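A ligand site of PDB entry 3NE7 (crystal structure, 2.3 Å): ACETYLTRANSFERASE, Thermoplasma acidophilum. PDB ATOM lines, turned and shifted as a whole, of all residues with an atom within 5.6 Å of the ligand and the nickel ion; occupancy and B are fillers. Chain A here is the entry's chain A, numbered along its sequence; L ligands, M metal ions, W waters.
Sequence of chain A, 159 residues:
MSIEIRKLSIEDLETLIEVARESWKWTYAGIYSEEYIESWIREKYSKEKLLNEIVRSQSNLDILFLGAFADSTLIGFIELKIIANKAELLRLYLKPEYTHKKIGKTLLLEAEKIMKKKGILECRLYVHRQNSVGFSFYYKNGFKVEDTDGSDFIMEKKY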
ATOM      1  N   SER A  23     -26.419  16.696  15.232  1.00  0.00           N
ATOM      2  CA  SER A  23     -25.261  16.279  14.445  1.00  0.00           C
ATOM      3  C   SER A  23     -24.397  17.476  14.088  1.00  0.00           C
ATOM      4  O   SER A  23     -23.170  17.463  14.243  1.00  0.00           O
ATOM      5  CB  SER A  23     -25.712  15.519  13.215  1.00  0.00           C
ATOM      6  OG  SER A  23     -24.671  14.790  12.610  1.00  0.00           O
ATOM      7  N   TRP A  26     -22.189  18.786  17.014  1.00  0.00           N
ATOM      8  CA  TRP A  26     -21.068  17.896  17.250  1.00  0.00           C
ATOM      9  C   TRP A  26     -20.023  17.966  16.133  1.00  0.00           C
ATOM     10  O   TRP A  26     -18.834  18.068  16.393  1.00  0.00           O
ATOM     11  CB  TRP A  26     -21.628  16.471  17.346  1.00  0.00           C
ATOM     12  CG  TRP A  26     -20.653  15.427  17.652  1.00  0.00           C
ATOM     13  CD1 TRP A  26     -20.063  15.199  18.857  1.00  0.00           C
ATOM     14  CD2 TRP A  26     -20.188  14.413  16.766  1.00  0.00           C
ATOM     15  NE1 TRP A  26     -19.221  14.101  18.764  1.00  0.00           N
ATOM     16  CE2 TRP A  26     -19.297  13.590  17.497  1.00  0.00           C
ATOM     17  CE3 TRP A  26     -20.435  14.110  15.431  1.00  0.00           C
ATOM     18  CZ2 TRP A  26     -18.612  12.514  16.932  1.00  0.00           C
ATOM     19  CZ3 TRP A  26     -19.788  13.014  14.858  1.00  0.00           C
ATOM     20  CH2 TRP A  26     -18.867  12.233  15.620  1.00  0.00           C
ATOM     21  N   THR A  27     -20.495  17.885  14.888  1.00  0.00           N
ATOM     22  CA  THR A  27     -19.609  17.819  13.738  1.00  0.00           C
ATOM     23  C   THR A  27     -18.741  19.102  13.596  1.00  0.00           C
ATOM     24  O   THR A  27     -17.548  19.027  13.280  1.00  0.00           O
ATOM     25  CB  THR A  27     -20.467  17.677  12.431  1.00  0.00           C
ATOM     26  OG1 THR A  27     -21.249  16.475  12.512  1.00  0.00           O
ATOM     27  CG2 THR A  27     -19.627  17.638  11.193  1.00  0.00           C
ATOM     28  N   TYR A  28     -19.341  20.249  13.847  1.00  0.00           N
ATOM     29  CA  TYR A  28     -18.665  21.535  13.599  1.00  0.00           C
ATOM     30  C   TYR A  28     -18.161  22.213  14.853  1.00  0.00           C
ATOM     31  O   TYR A  28     -17.809  23.376  14.794  1.00  0.00           O
ATOM     32  CB  TYR A  28     -19.572  22.457  12.800  1.00  0.00           C
ATOM     33  CG  TYR A  28     -19.932  21.831  11.469  1.00  0.00           C
ATOM     34  CD1 TYR A  28     -18.976  21.692  10.469  1.00  0.00           C
ATOM     35  CD2 TYR A  28     -21.179  21.336  11.244  1.00  0.00           C
ATOM     36  CE1 TYR A  28     -19.301  21.086   9.252  1.00  0.00           C
ATOM     37  CE2 TYR A  28     -21.511  20.731  10.057  1.00  0.00           C
ATOM     38  CZ  TYR A  28     -20.573  20.598   9.053  1.00  0.00           C
ATOM     39  OH  TYR A  28     -20.972  19.953   7.863  1.00  0.00           O
ATOM     40  N   LEU A  90     -26.015  16.274  -0.815  1.00  0.00           N
ATOM     41  CA  LEU A  90     -26.187  17.493  -0.001  1.00  0.00           C
ATOM     42  C   LEU A  90     -25.901  17.322   1.493  1.00  0.00           C
ATOM     43  O   LEU A  90     -25.278  18.190   2.129  1.00  0.00           O
ATOM     44  CB  LEU A  90     -27.627  17.981  -0.109  1.00  0.00           C
ATOM     45  CG  LEU A  90     -28.099  18.449  -1.471  1.00  0.00           C
ATOM     46  CD1 LEU A  90     -29.550  18.897  -1.354  1.00  0.00           C
ATOM     47  CD2 LEU A  90     -27.182  19.598  -1.987  1.00  0.00           C
ATOM     48  N   LEU A  92     -25.629  14.293   4.926  1.00  0.00           N
ATOM     49  CA  LEU A  92     -25.556  12.993   5.524  1.00  0.00           C
ATOM     50  C   LEU A  92     -25.137  13.234   6.963  1.00  0.00           C
ATOM     51  O   LEU A  92     -23.997  13.605   7.231  1.00  0.00           O
ATOM     52  CB  LEU A  92     -24.520  12.154   4.776  1.00  0.00           C
ATOM     53  CG  LEU A  92     -24.219  10.749   5.264  1.00  0.00           C
ATOM     54  CD1 LEU A  92     -25.473   9.908   5.446  1.00  0.00           C
ATOM     55  CD2 LEU A  92     -23.208  10.051   4.315  1.00  0.00           C
ATOM     56  N   TYR A  93     -26.065  13.036   7.892  1.00  0.00           N
ATOM     57  CA  TYR A  93     -25.850  13.347   9.285  1.00  0.00           C
ATOM     58  C   TYR A  93     -26.494  12.246  10.111  1.00  0.00           C
ATOM     59  O   TYR A  93     -27.653  11.844   9.831  1.00  0.00           O
ATOM     60  CB  TYR A  93     -26.456  14.732   9.644  1.00  0.00           C
ATOM     61  CG  TYR A  93     -25.746  15.914   8.989  1.00  0.00           C
ATOM     62  CD1 TYR A  93     -24.578  16.445   9.523  1.00  0.00           C
ATOM     63  CD2 TYR A  93     -26.199  16.446   7.788  1.00  0.00           C
ATOM     64  CE1 TYR A  93     -23.896  17.498   8.888  1.00  0.00           C
ATOM     65  CE2 TYR A  93     -25.536  17.509   7.158  1.00  0.00           C
ATOM     66  CZ  TYR A  93     -24.390  18.020   7.708  1.00  0.00           C
ATOM     67  OH  TYR A  93     -23.716  19.040   7.062  1.00  0.00           O
ATOM     68  N   LEU A  94     -25.782  11.794  11.152  1.00  0.00           N
ATOM     69  CA  LEU A  94     -26.310  10.848  12.127  1.00  0.00           C
ATOM     70  C   LEU A  94     -26.275  11.513  13.474  1.00  0.00           C
ATOM     71  O   LEU A  94     -25.432  12.361  13.683  1.00  0.00           O
ATOM     72  CB  LEU A  94     -25.427   9.601  12.196  1.00  0.00           C
ATOM     73  CG  LEU A  94     -25.139   8.791  10.923  1.00  0.00           C
ATOM     74  CD1 LEU A  94     -24.329   7.496  11.288  1.00  0.00           C
ATOM     75  CD2 LEU A  94     -26.411   8.420  10.184  1.00  0.00           C
ATOM     76  N   PRO A  96     -24.800  11.736  16.967  1.00  0.00           N
ATOM     77  CA  PRO A  96     -23.414  11.433  17.314  1.00  0.00           C
ATOM     78  C   PRO A  96     -23.201  10.031  17.952  1.00  0.00           C
ATOM     79  O   PRO A  96     -22.293   9.350  17.582  1.00  0.00           O
ATOM     80  CB  PRO A  96     -23.055  12.584  18.260  1.00  0.00           C
ATOM     81  CG  PRO A  96     -23.832  13.703  17.768  1.00  0.00           C
ATOM     82  CD  PRO A  96     -25.127  13.149  17.282  1.00  0.00           C
ATOM     83  N   TYR A  98     -24.878   7.364  17.394  1.00  0.00           N
ATOM     84  CA  TYR A  98     -25.125   6.324  16.410  1.00  0.00           C
ATOM     85  C   TYR A  98     -24.048   6.291  15.332  1.00  0.00           C
ATOM     86  O   TYR A  98     -24.161   5.529  14.373  1.00  0.00           O
ATOM     87  CB  TYR A  98     -26.526   6.524  15.778  1.00  0.00           C
ATOM     88  CG  TYR A  98     -27.626   6.086  16.719  1.00  0.00           C
ATOM     89  CD1 TYR A  98     -28.075   4.768  16.726  1.00  0.00           C
ATOM     90  CD2 TYR A  98     -28.155   6.952  17.660  1.00  0.00           C
ATOM     91  CE1 TYR A  98     -29.085   4.348  17.628  1.00  0.00           C
ATOM     92  CE2 TYR A  98     -29.162   6.559  18.542  1.00  0.00           C
ATOM     93  CZ  TYR A  98     -29.611   5.255  18.523  1.00  0.00           C
ATOM     94  OH  TYR A  98     -30.578   4.843  19.394  1.00  0.00           O
ATOM     95  N   THR A  99     -22.993   7.106  15.458  1.00  0.00           N
ATOM     96  CA  THR A  99     -21.932   7.067  14.488  1.00  0.00           C
ATOM     97  C   THR A  99     -21.038   5.844  14.687  1.00  0.00           C
ATOM     98  O   THR A  99     -21.066   5.231  15.738  1.00  0.00           O
ATOM     99  CB  THR A  99     -21.065   8.347  14.485  1.00  0.00           C
ATOM    100  OG1 THR A  99     -20.465   8.513  15.777  1.00  0.00           O
ATOM    101  CG2 THR A  99     -21.922   9.555  14.102  1.00  0.00           C
ATOM    102  N   HIS A 100     -20.267   5.492  13.657  1.00  0.00           N
ATOM    103  CA  HIS A 100     -19.220   4.448  13.694  1.00  0.00           C
ATOM    104  C   HIS A 100     -19.849   3.066  13.874  1.00  0.00           C
ATOM    105  O   HIS A 100     -19.237   2.152  14.405  1.00  0.00           O
ATOM    106  CB  HIS A 100     -18.191   4.759  14.790  1.00  0.00           C
ATOM    107  CG  HIS A 100     -16.798   4.233  14.523  1.00  0.00           C
ATOM    108  ND1 HIS A 100     -16.487   2.887  14.481  1.00  0.00           N
ATOM    109  CD2 HIS A 100     -15.615   4.883  14.358  1.00  0.00           C
ATOM    110  CE1 HIS A 100     -15.198   2.743  14.252  1.00  0.00           C
ATOM    111  NE2 HIS A 100     -14.642   3.937  14.204  1.00  0.00           N
ATOM    112  N   LYS A 101     -21.069   2.888  13.393  1.00  0.00           N
ATOM    113  CA  LYS A 101     -21.694   1.568  13.414  1.00  0.00           C
ATOM    114  C   LYS A 101     -22.181   1.188  12.016  1.00  0.00           C
ATOM    115  O   LYS A 101     -22.972   0.279  11.865  1.00  0.00           O
ATOM    116  CB  LYS A 101     -22.850   1.544  14.418  1.00  0.00           C
ATOM    117  CG  LYS A 101     -22.421   1.938  15.858  1.00  0.00           C
ATOM    118  CD  LYS A 101     -23.612   2.352  16.737  1.00  0.00           C
ATOM    119  CE  LYS A 101     -23.182   3.045  18.052  1.00  0.00           C
ATOM    120  NZ  LYS A 101     -22.692   2.084  19.151  1.00  0.00           N
ATOM    121  N   LYS A 102     -21.666   1.896  11.015  1.00  0.00           N
ATOM    122  CA  LYS A 102     -21.967   1.634   9.595  1.00  0.00           C
ATOM    123  C   LYS A 102     -23.361   2.017   9.167  1.00  0.00           C
ATOM    124  O   LYS A 102     -23.839   1.599   8.102  1.00  0.00           O
ATOM    125  CB  LYS A 102     -21.626   0.183   9.210  1.00  0.00           C
ATOM    126  CG  LYS A 102     -20.131  -0.081   9.278  1.00  0.00           C
ATOM    127  CD  LYS A 102     -19.786  -1.521   9.082  1.00  0.00           C
ATOM    128  CE  LYS A 102     -18.388  -1.810   9.637  1.00  0.00           C
ATOM    129  NZ  LYS A 102     -17.531  -0.627   9.338  1.00  0.00           N
ATOM    130  N   ILE A 103     -24.039   2.820   9.955  1.00  0.00           N
ATOM    131  CA  ILE A 103     -25.363   3.291   9.545  1.00  0.00           C
ATOM    132  C   ILE A 103     -25.228   4.301   8.389  1.00  0.00           C
ATOM    133  O   ILE A 103     -26.035   4.293   7.445  1.00  0.00           O
ATOM    134  CB  ILE A 103     -26.132   3.900  10.721  1.00  0.00           C
ATOM    135  CG1 ILE A 103     -26.408   2.795  11.778  1.00  0.00           C
ATOM    136  CG2 ILE A 103     -27.460   4.548  10.218  1.00  0.00           C
ATOM    137  CD1 ILE A 103     -26.888   3.260  13.130  1.00  0.00           C
ATOM    138  N   GLY A 104     -24.189   5.125   8.414  1.00  0.00           N
ATOM    139  CA  GLY A 104     -23.968   6.052   7.328  1.00  0.00           C
ATOM    140  C   GLY A 104     -23.547   5.377   6.053  1.00  0.00           C
ATOM    141  O   GLY A 104     -23.936   5.793   4.964  1.00  0.00           O
ATOM    142  N   LYS A 105     -22.751   4.318   6.175  1.00  0.00           N
ATOM    143  CA  LYS A 105     -22.362   3.535   5.020  1.00  0.00           C
ATOM    144  C   LYS A 105     -23.603   2.949   4.391  1.00  0.00           C
ATOM    145  O   LYS A 105     -23.761   2.985   3.181  1.00  0.00           O
ATOM    146  CB  LYS A 105     -21.391   2.425   5.434  1.00  0.00           C
ATOM    147  CG  LYS A 105     -20.758   1.650   4.270  1.00  0.00           C
ATOM    148  CD  LYS A 105     -19.920   0.486   4.805  1.00  0.00           C
ATOM    149  CE  LYS A 105     -18.903  -0.006   3.764  1.00  0.00           C
ATOM    150  NZ  LYS A 105     -17.757   0.981   3.659  1.00  0.00           N
ATOM    151  N   TYR A 126     -19.643  18.259  -1.292  1.00  0.00           N
ATOM    152  CA  TYR A 126     -18.814  19.309  -0.665  1.00  0.00           C
ATOM    153  C   TYR A 126     -18.586  18.985   0.801  1.00  0.00           C
ATOM    154  O   TYR A 126     -19.538  18.772   1.573  1.00  0.00           O
ATOM    155  CB  TYR A 126     -19.512  20.672  -0.798  1.00  0.00           C
ATOM    156  CG  TYR A 126     -19.500  21.251  -2.211  1.00  0.00           C
ATOM    157  CD1 TYR A 126     -18.717  22.390  -2.535  1.00  0.00           C
ATOM    158  CD2 TYR A 126     -20.262  20.676  -3.219  1.00  0.00           C
ATOM    159  CE1 TYR A 126     -18.713  22.926  -3.838  1.00  0.00           C
ATOM    160  CE2 TYR A 126     -20.274  21.194  -4.528  1.00  0.00           C
ATOM    161  CZ  TYR A 126     -19.495  22.310  -4.824  1.00  0.00           C
ATOM    162  OH  TYR A 126     -19.539  22.799  -6.126  1.00  0.00           O
ATOM    163  N   VAL A 127     -17.330  18.877   1.205  1.00  0.00           N
ATOM    164  CA  VAL A 127     -17.037  18.574   2.607  1.00  0.00           C
ATOM    165  C   VAL A 127     -16.041  19.580   3.096  1.00  0.00           C
ATOM    166  O   VAL A 127     -15.052  19.842   2.428  1.00  0.00           O
ATOM    167  CB  VAL A 127     -16.523  17.141   2.776  1.00  0.00           C
ATOM    168  CG1 VAL A 127     -15.224  16.894   1.967  1.00  0.00           C
ATOM    169  CG2 VAL A 127     -16.344  16.825   4.277  1.00  0.00           C
ATOM    170  N   ASN A 131     -13.391  18.963   8.579  1.00  0.00           N
ATOM    171  CA  ASN A 131     -14.235  17.874   9.060  1.00  0.00           C
ATOM    172  C   ASN A 131     -13.635  16.509   8.758  1.00  0.00           C
ATOM    173  O   ASN A 131     -13.983  15.843   7.793  1.00  0.00           O
ATOM    174  CB  ASN A 131     -15.646  17.997   8.497  1.00  0.00           C
ATOM    175  CG  ASN A 131     -16.528  16.869   8.945  1.00  0.00           C
ATOM    176  OD1 ASN A 131     -16.168  16.072   9.814  1.00  0.00           O
ATOM    177  ND2 ASN A 131     -17.691  16.777   8.344  1.00  0.00           N
ATOM    178  N   SER A 132     -12.679  16.096   9.597  1.00  0.00           N
ATOM    179  CA  SER A 132     -12.006  14.822   9.399  1.00  0.00           C
ATOM    180  C   SER A 132     -12.930  13.593   9.495  1.00  0.00           C
ATOM    181  O   SER A 132     -12.653  12.561   8.883  1.00  0.00           O
ATOM    182  CB  SER A 132     -10.879  14.708  10.418  1.00  0.00           C
ATOM    183  OG  SER A 132      -9.895  15.634  10.073  1.00  0.00           O
ATOM    184  N   VAL A 133     -13.970  13.692  10.319  1.00  0.00           N
ATOM    185  CA  VAL A 133     -14.902  12.581  10.533  1.00  0.00           C
ATOM    186  C   VAL A 133     -15.562  12.264   9.180  1.00  0.00           C
ATOM    187  O   VAL A 133     -15.436  11.165   8.660  1.00  0.00           O
ATOM    188  CB  VAL A 133     -15.969  12.913  11.646  1.00  0.00           C
ATOM    189  CG1 VAL A 133     -17.061  11.883  11.687  1.00  0.00           C
ATOM    190  CG2 VAL A 133     -15.278  13.047  13.108  1.00  0.00           C
ATOM    191  N   GLY A 134     -16.224  13.251   8.597  1.00  0.00           N
ATOM    192  CA  GLY A 134     -16.833  13.055   7.303  1.00  0.00           C
ATOM    193  C   GLY A 134     -15.874  12.773   6.172  1.00  0.00           C
ATOM    194  O   GLY A 134     -16.122  11.876   5.362  1.00  0.00           O
ATOM    195  N   SER A 136     -12.846  11.508   6.154  1.00  0.00           N
ATOM    196  CA  SER A 136     -12.269  10.153   6.260  1.00  0.00           C
ATOM    197  C   SER A 136     -13.329   9.113   5.904  1.00  0.00           C
ATOM    198  O   SER A 136     -13.060   8.127   5.211  1.00  0.00           O
ATOM    199  CB  SER A 136     -11.679   9.930   7.666  1.00  0.00           C
ATOM    200  OG  SER A 136     -12.716   9.881   8.638  1.00  0.00           O
ATOM    201  N   PHE A 137     -14.558   9.319   6.341  1.00  0.00           N
ATOM    202  CA  PHE A 137     -15.614   8.389   5.947  1.00  0.00           C
ATOM    203  C   PHE A 137     -15.778   8.300   4.428  1.00  0.00           C
ATOM    204  O   PHE A 137     -15.936   7.189   3.851  1.00  0.00           O
ATOM    205  CB  PHE A 137     -16.914   8.765   6.626  1.00  0.00           C
ATOM    206  CG  PHE A 137     -18.151   8.134   6.003  1.00  0.00           C
ATOM    207  CD1 PHE A 137     -18.892   8.840   5.052  1.00  0.00           C
ATOM    208  CD2 PHE A 137     -18.560   6.853   6.373  1.00  0.00           C
ATOM    209  CE1 PHE A 137     -20.048   8.295   4.492  1.00  0.00           C
ATOM    210  CE2 PHE A 137     -19.715   6.291   5.830  1.00  0.00           C
ATOM    211  CZ  PHE A 137     -20.470   6.995   4.889  1.00  0.00           C
ATOM    212  N   TYR A 138     -15.731   9.478   3.779  1.00  0.00           N
ATOM    213  CA  TYR A 138     -15.853   9.528   2.334  1.00  0.00           C
ATOM    214  C   TYR A 138     -14.747   8.847   1.570  1.00  0.00           C
ATOM    215  O   TYR A 138     -15.026   8.096   0.642  1.00  0.00           O
ATOM    216  CB  TYR A 138     -16.008  10.971   1.837  1.00  0.00           C
ATOM    217  CG  TYR A 138     -17.367  11.538   2.210  1.00  0.00           C
ATOM    218  CD1 TYR A 138     -18.508  10.791   2.041  1.00  0.00           C
ATOM    219  CD2 TYR A 138     -17.491  12.812   2.754  1.00  0.00           C
ATOM    220  CE1 TYR A 138     -19.788  11.312   2.374  1.00  0.00           C
ATOM    221  CE2 TYR A 138     -18.736  13.341   3.088  1.00  0.00           C
ATOM    222  CZ  TYR A 138     -19.887  12.579   2.891  1.00  0.00           C
ATOM    223  OH  TYR A 138     -21.152  13.100   3.205  1.00  0.00           O
ATOM    224  N   LYS A 140     -12.891   6.499   2.677  1.00  0.00           N
ATOM    225  CA  LYS A 140     -13.012   5.064   2.972  1.00  0.00           C
ATOM    226  C   LYS A 140     -14.151   4.445   2.227  1.00  0.00           C
ATOM    227  O   LYS A 140     -14.253   3.250   2.227  1.00  0.00           O
ATOM    228  CB  LYS A 140     -13.128   4.790   4.502  1.00  0.00           C
ATOM    229  CG  LYS A 140     -11.783   4.942   5.250  1.00  0.00           C
ATOM    230  CD  LYS A 140     -11.941   5.235   6.738  1.00  0.00           C
ATOM    231  CE  LYS A 140     -10.627   5.638   7.385  1.00  0.00           C
ATOM    232  NZ  LYS A 140     -10.781   5.814   8.861  1.00  0.00           N
ATOM    233  N   ASN A 141     -15.009   5.237   1.585  1.00  0.00           N
ATOM    234  CA  ASN A 141     -16.088   4.735   0.752  1.00  0.00           C
ATOM    235  C   ASN A 141     -15.912   5.127  -0.717  1.00  0.00           C
ATOM    236  O   ASN A 141     -16.898   5.231  -1.464  1.00  0.00           O
ATOM    237  CB  ASN A 141     -17.415   5.215   1.328  1.00  0.00           C
ATOM    238  CG  ASN A 141     -17.805   4.422   2.553  1.00  0.00           C
ATOM    239  OD1 ASN A 141     -18.154   3.249   2.435  1.00  0.00           O
ATOM    240  ND2 ASN A 141     -17.652   5.011   3.737  1.00  0.00           N
HETATM  241  N1  LIG L   1     -15.275   9.634  15.317  1.00  0.00           N
HETATM  242  C1  LIG L   1     -14.273   9.649  14.406  1.00  0.00           C
HETATM  243  N2  LIG L   1     -14.400   9.101  13.168  1.00  0.00           N
HETATM  244  C2  LIG L   1     -15.588   8.511  12.823  1.00  0.00           C
HETATM  245  C3  LIG L   1     -16.675   8.488  13.812  1.00  0.00           C
HETATM  246  C4  LIG L   1     -16.474   9.061  15.049  1.00  0.00           C
HETATM  247  N3  LIG L   1     -17.457   9.043  15.973  1.00  0.00           N
HETATM  248  N4  LIG L   1     -17.709   7.877  13.235  1.00  0.00           N
HETATM  249  C5  LIG L   1     -17.334   7.520  11.984  1.00  0.00           C
HETATM  250  N5  LIG L   1     -16.073   7.894  11.720  1.00  0.00           N
HETATM  251  C6  LIG L   1     -15.383   7.697  10.425  1.00  0.00           C
HETATM  252  C7  LIG L   1     -13.999   7.072  10.522  1.00  0.00           C
HETATM  253  O1  LIG L   1     -13.200   7.492   9.407  1.00  0.00           O
HETATM  254  C8  LIG L   1     -14.385   5.595  10.537  1.00  0.00           C
HETATM  255  O2  LIG L   1     -13.401   4.685  10.149  1.00  0.00           O
HETATM  256  P1  LIG L   1     -12.455   3.968  11.231  1.00  0.00           P
HETATM  257  O3  LIG L   1     -13.174   2.698  11.693  1.00  0.00           O
HETATM  258  O4  LIG L   1     -12.192   4.965  12.317  1.00  0.00           O
HETATM  259  O5  LIG L   1     -11.270   3.678  10.382  1.00  0.00           O
HETATM  260  C9  LIG L   1     -15.569   5.531   9.594  1.00  0.00           C
HETATM  261  O6  LIG L   1     -16.156   6.831   9.591  1.00  0.00           O
HETATM  262  C10 LIG L   1     -16.587   4.482  10.044  1.00  0.00           C
HETATM  263  O7  LIG L   1     -17.571   4.341   9.010  1.00  0.00           O
HETATM  264  P2  LIG L   1     -19.100   4.159   9.317  1.00  0.00           P
HETATM  265  O8  LIG L   1     -19.303   3.424  10.615  1.00  0.00           O
HETATM  266  O9  LIG L   1     -19.645   3.610   8.057  1.00  0.00           O
HETATM  267  O10 LIG L   1     -19.536   5.699   9.491  1.00  0.00           O
HETATM  268  P3  LIG L   1     -20.912   6.292  10.077  1.00  0.00           P
HETATM  269  O11 LIG L   1     -20.561   7.023  11.370  1.00  0.00           O
HETATM  270  O12 LIG L   1     -21.984   5.198  10.121  1.00  0.00           O
HETATM  271  O13 LIG L   1     -21.318   7.436   9.030  1.00  0.00           O
HETATM  272  C11 LIG L   1     -20.868   9.836   8.955  1.00  0.00           C
HETATM  273  C12 LIG L   1     -20.344   8.455   8.682  1.00  0.00           C
HETATM  274  C13 LIG L   1     -19.912  10.907   8.385  1.00  0.00           C
HETATM  275  C14 LIG L   1     -22.195   9.969   8.280  1.00  0.00           C
HETATM  276  C15 LIG L   1     -21.163   9.967  10.464  1.00  0.00           C
HETATM  277  O14 LIG L   1     -19.973   9.661  11.196  1.00  0.00           O
HETATM  278  C16 LIG L   1     -21.679  11.370  10.784  1.00  0.00           C
HETATM  279  O15 LIG L   1     -22.888  11.603  10.746  1.00  0.00           O
HETATM  280  N6  LIG L   1     -20.789  12.316  11.080  1.00  0.00           N
HETATM  281  C17 LIG L   1     -21.075  13.708  11.418  1.00  0.00           C
HETATM  282  C18 LIG L   1     -21.633  14.515  10.238  1.00  0.00           C
HETATM  283  C19 LIG L   1     -20.714  14.528   9.021  1.00  0.00           C
HETATM  284  O16 LIG L   1     -19.497  14.692   9.156  1.00  0.00           O
HETATM  285  N7  LIG L   1     -21.339  14.348   7.869  1.00  0.00           N
HETATM  286  C20 LIG L   1     -20.877  14.218   6.484  1.00  0.00           C
HETATM  287  C21 LIG L   1     -20.236  15.527   6.043  1.00  0.00           C
HETATM  288  S1  LIG L   1     -21.460  16.846   5.966  1.00  0.00           S
HETATM  289 NI    NI M   1     -12.740   4.575  14.097  1.00  0.00          NI
HETATM  290  O   HOH W   1     -23.200   4.351  12.330  1.00  0.00           O
HETATM  291  O   HOH W   2     -12.015   0.332  11.936  1.00  0.00           O
HETATM  292  O   HOH W   3     -10.390   6.779  11.684  1.00  0.00           O
HETATM  293  O   HOH W   4     -12.309  10.288  11.869  1.00  0.00           O
HETATM  294  O   HOH W   5     -11.393   1.589   8.670  1.00  0.00           O
HETATM  295  O   HOH W   6     -15.119   1.383  10.999  1.00  0.00           O
HETATM  296  O   HOH W   7     -17.755   1.433  11.439  1.00  0.00           O
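The side-chain amino group (NZ) of Lys 140 is in salt-bridge range of an oxygen (O5) of the ligand (2.7 Å).
N of Lys 101 is in hydrogen-bond range of O8 of the ligand.
The side-chain hydroxyl of Tyr 28 sits close to a sulfur (S1) of the ligand (3.7 Å).
O1 of the ligand is in hydrogen-bond range of OG of Ser 136, at 2.6 Å.
An oxygen (O8) of the ligand is in hydrogen-bond range of the backbone NH of Lys 102 (2.8 Å).
N of Gly 104 is in hydrogen-bond range of O12 of the ligand, 2.8 Å away.
An oxygen (O12) of the ligand lies within hydrogen-bond range of the backbone NH (N) of Ile 103 (3.1 Å).
An oxygen (O15) of the ligand lies within hydrogen-bond range of the backbone NH of Leu 94 (2.9 Å).
A sulfur (S1) of the ligand sits close to the side-chain hydroxyl (OH) of Tyr 93, 3.3 Å away.
The side-chain amide nitrogen (ND2) of Asn 131 is in hydrogen-bond range of an oxygen (O16) of the ligand, 2.9 Å away.
The backbone NH (N) of His 100 is in hydrogen-bond range of an oxygen (O11) of the ligand, at 2.8 Å.
The backbone carbonyl oxygen (O) of Leu 92 lies within hydrogen-bond range of a nitrogen (N7) of the ligand, at 2.8 Å.
N3 of the ligand is in hydrogen-bond range of OG1 of Thr 99.
OG of Ser 136 is in hydrogen-bond range of O of Val 133 (3.0 Å).
OG of Ser 136 is in hydrogen-bond range of O of Ser 132 (2.7 Å).
The side-chain amide oxygen (OD1) of Asn 131 lies close to the backbone NH (N) of Val 133, at 3.3 Å.
The side-chain amide oxygen of Asn 131 lies within hydrogen-bond range of the backbone NH of Gly 134.
O of Ser 23 is in hydrogen-bond range of OG1 of Thr 27 (2.8 Å).
The side-chain hydroxyl (OH) of Tyr 93 lies within hydrogen-bond range of the side-chain hydroxyl (OH) of Tyr 28, 3.0 Å away.
The side-chain amino group (NZ) of Lys 105 lies within hydrogen-bond range of the side-chain amide oxygen (OD1) of Asn 141, 2.6 Å away.
The side-chain hydroxyl (OG1) of Thr 99 is in hydrogen-bond range of the backbone carbonyl oxygen (O) of Pro 96 (2.7 Å).
OG of Ser 23 touches C18 of the ligand (3.9 Å).
Trp 26 touches the ligand (CH2 to N3, 3.5 Å).
Thr 27 touches the ligand (OG1 to C17, 3.0 Å).
CB of Lys 105 touches O9 of the ligand (3.4 Å).
Val 133 touches the ligand (CG1 to O14, 3.7 Å).
Gly 134 touches the ligand (N to O16, 3.6 Å).
Phe 137 touches the ligand (CD2 to C12, 3.3 Å).
OH of Tyr 138 touches C20 of the ligand, 3.5 Å away.
Of the 28 residues printed, 21 come within 4 Å of the ligand.
Along chain A the residues within 4 Å of the ligand span positions 23 to 140.
Of the 28 residues printed, 1 comes within 4 Å of the nickel ion.
The nearest printed residue that does not touch the nickel ion is Lys 140 (5.7 Å).
The nickel ion is bound by O4 of the ligand (1.9 Å).
NE2 of His 100 is bound to the nickel ion.
Water W3 lies within hydrogen-bond range of the side-chain amino group of Lys 140 (3.0 Å) and an oxygen (O5) of the ligand (3.5 Å).
Water W7 lies within hydrogen-bond range of O8 of the ligand (2.7 Å), NZ of Lys 102 (3.0 Å) and O of His 100 (3.4 Å).
Water W4 bridges a nitrogen (N2) of the ligand (2.7 Å) and the side-chain hydroxyl (OG) of Ser 136 (3.3 Å).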
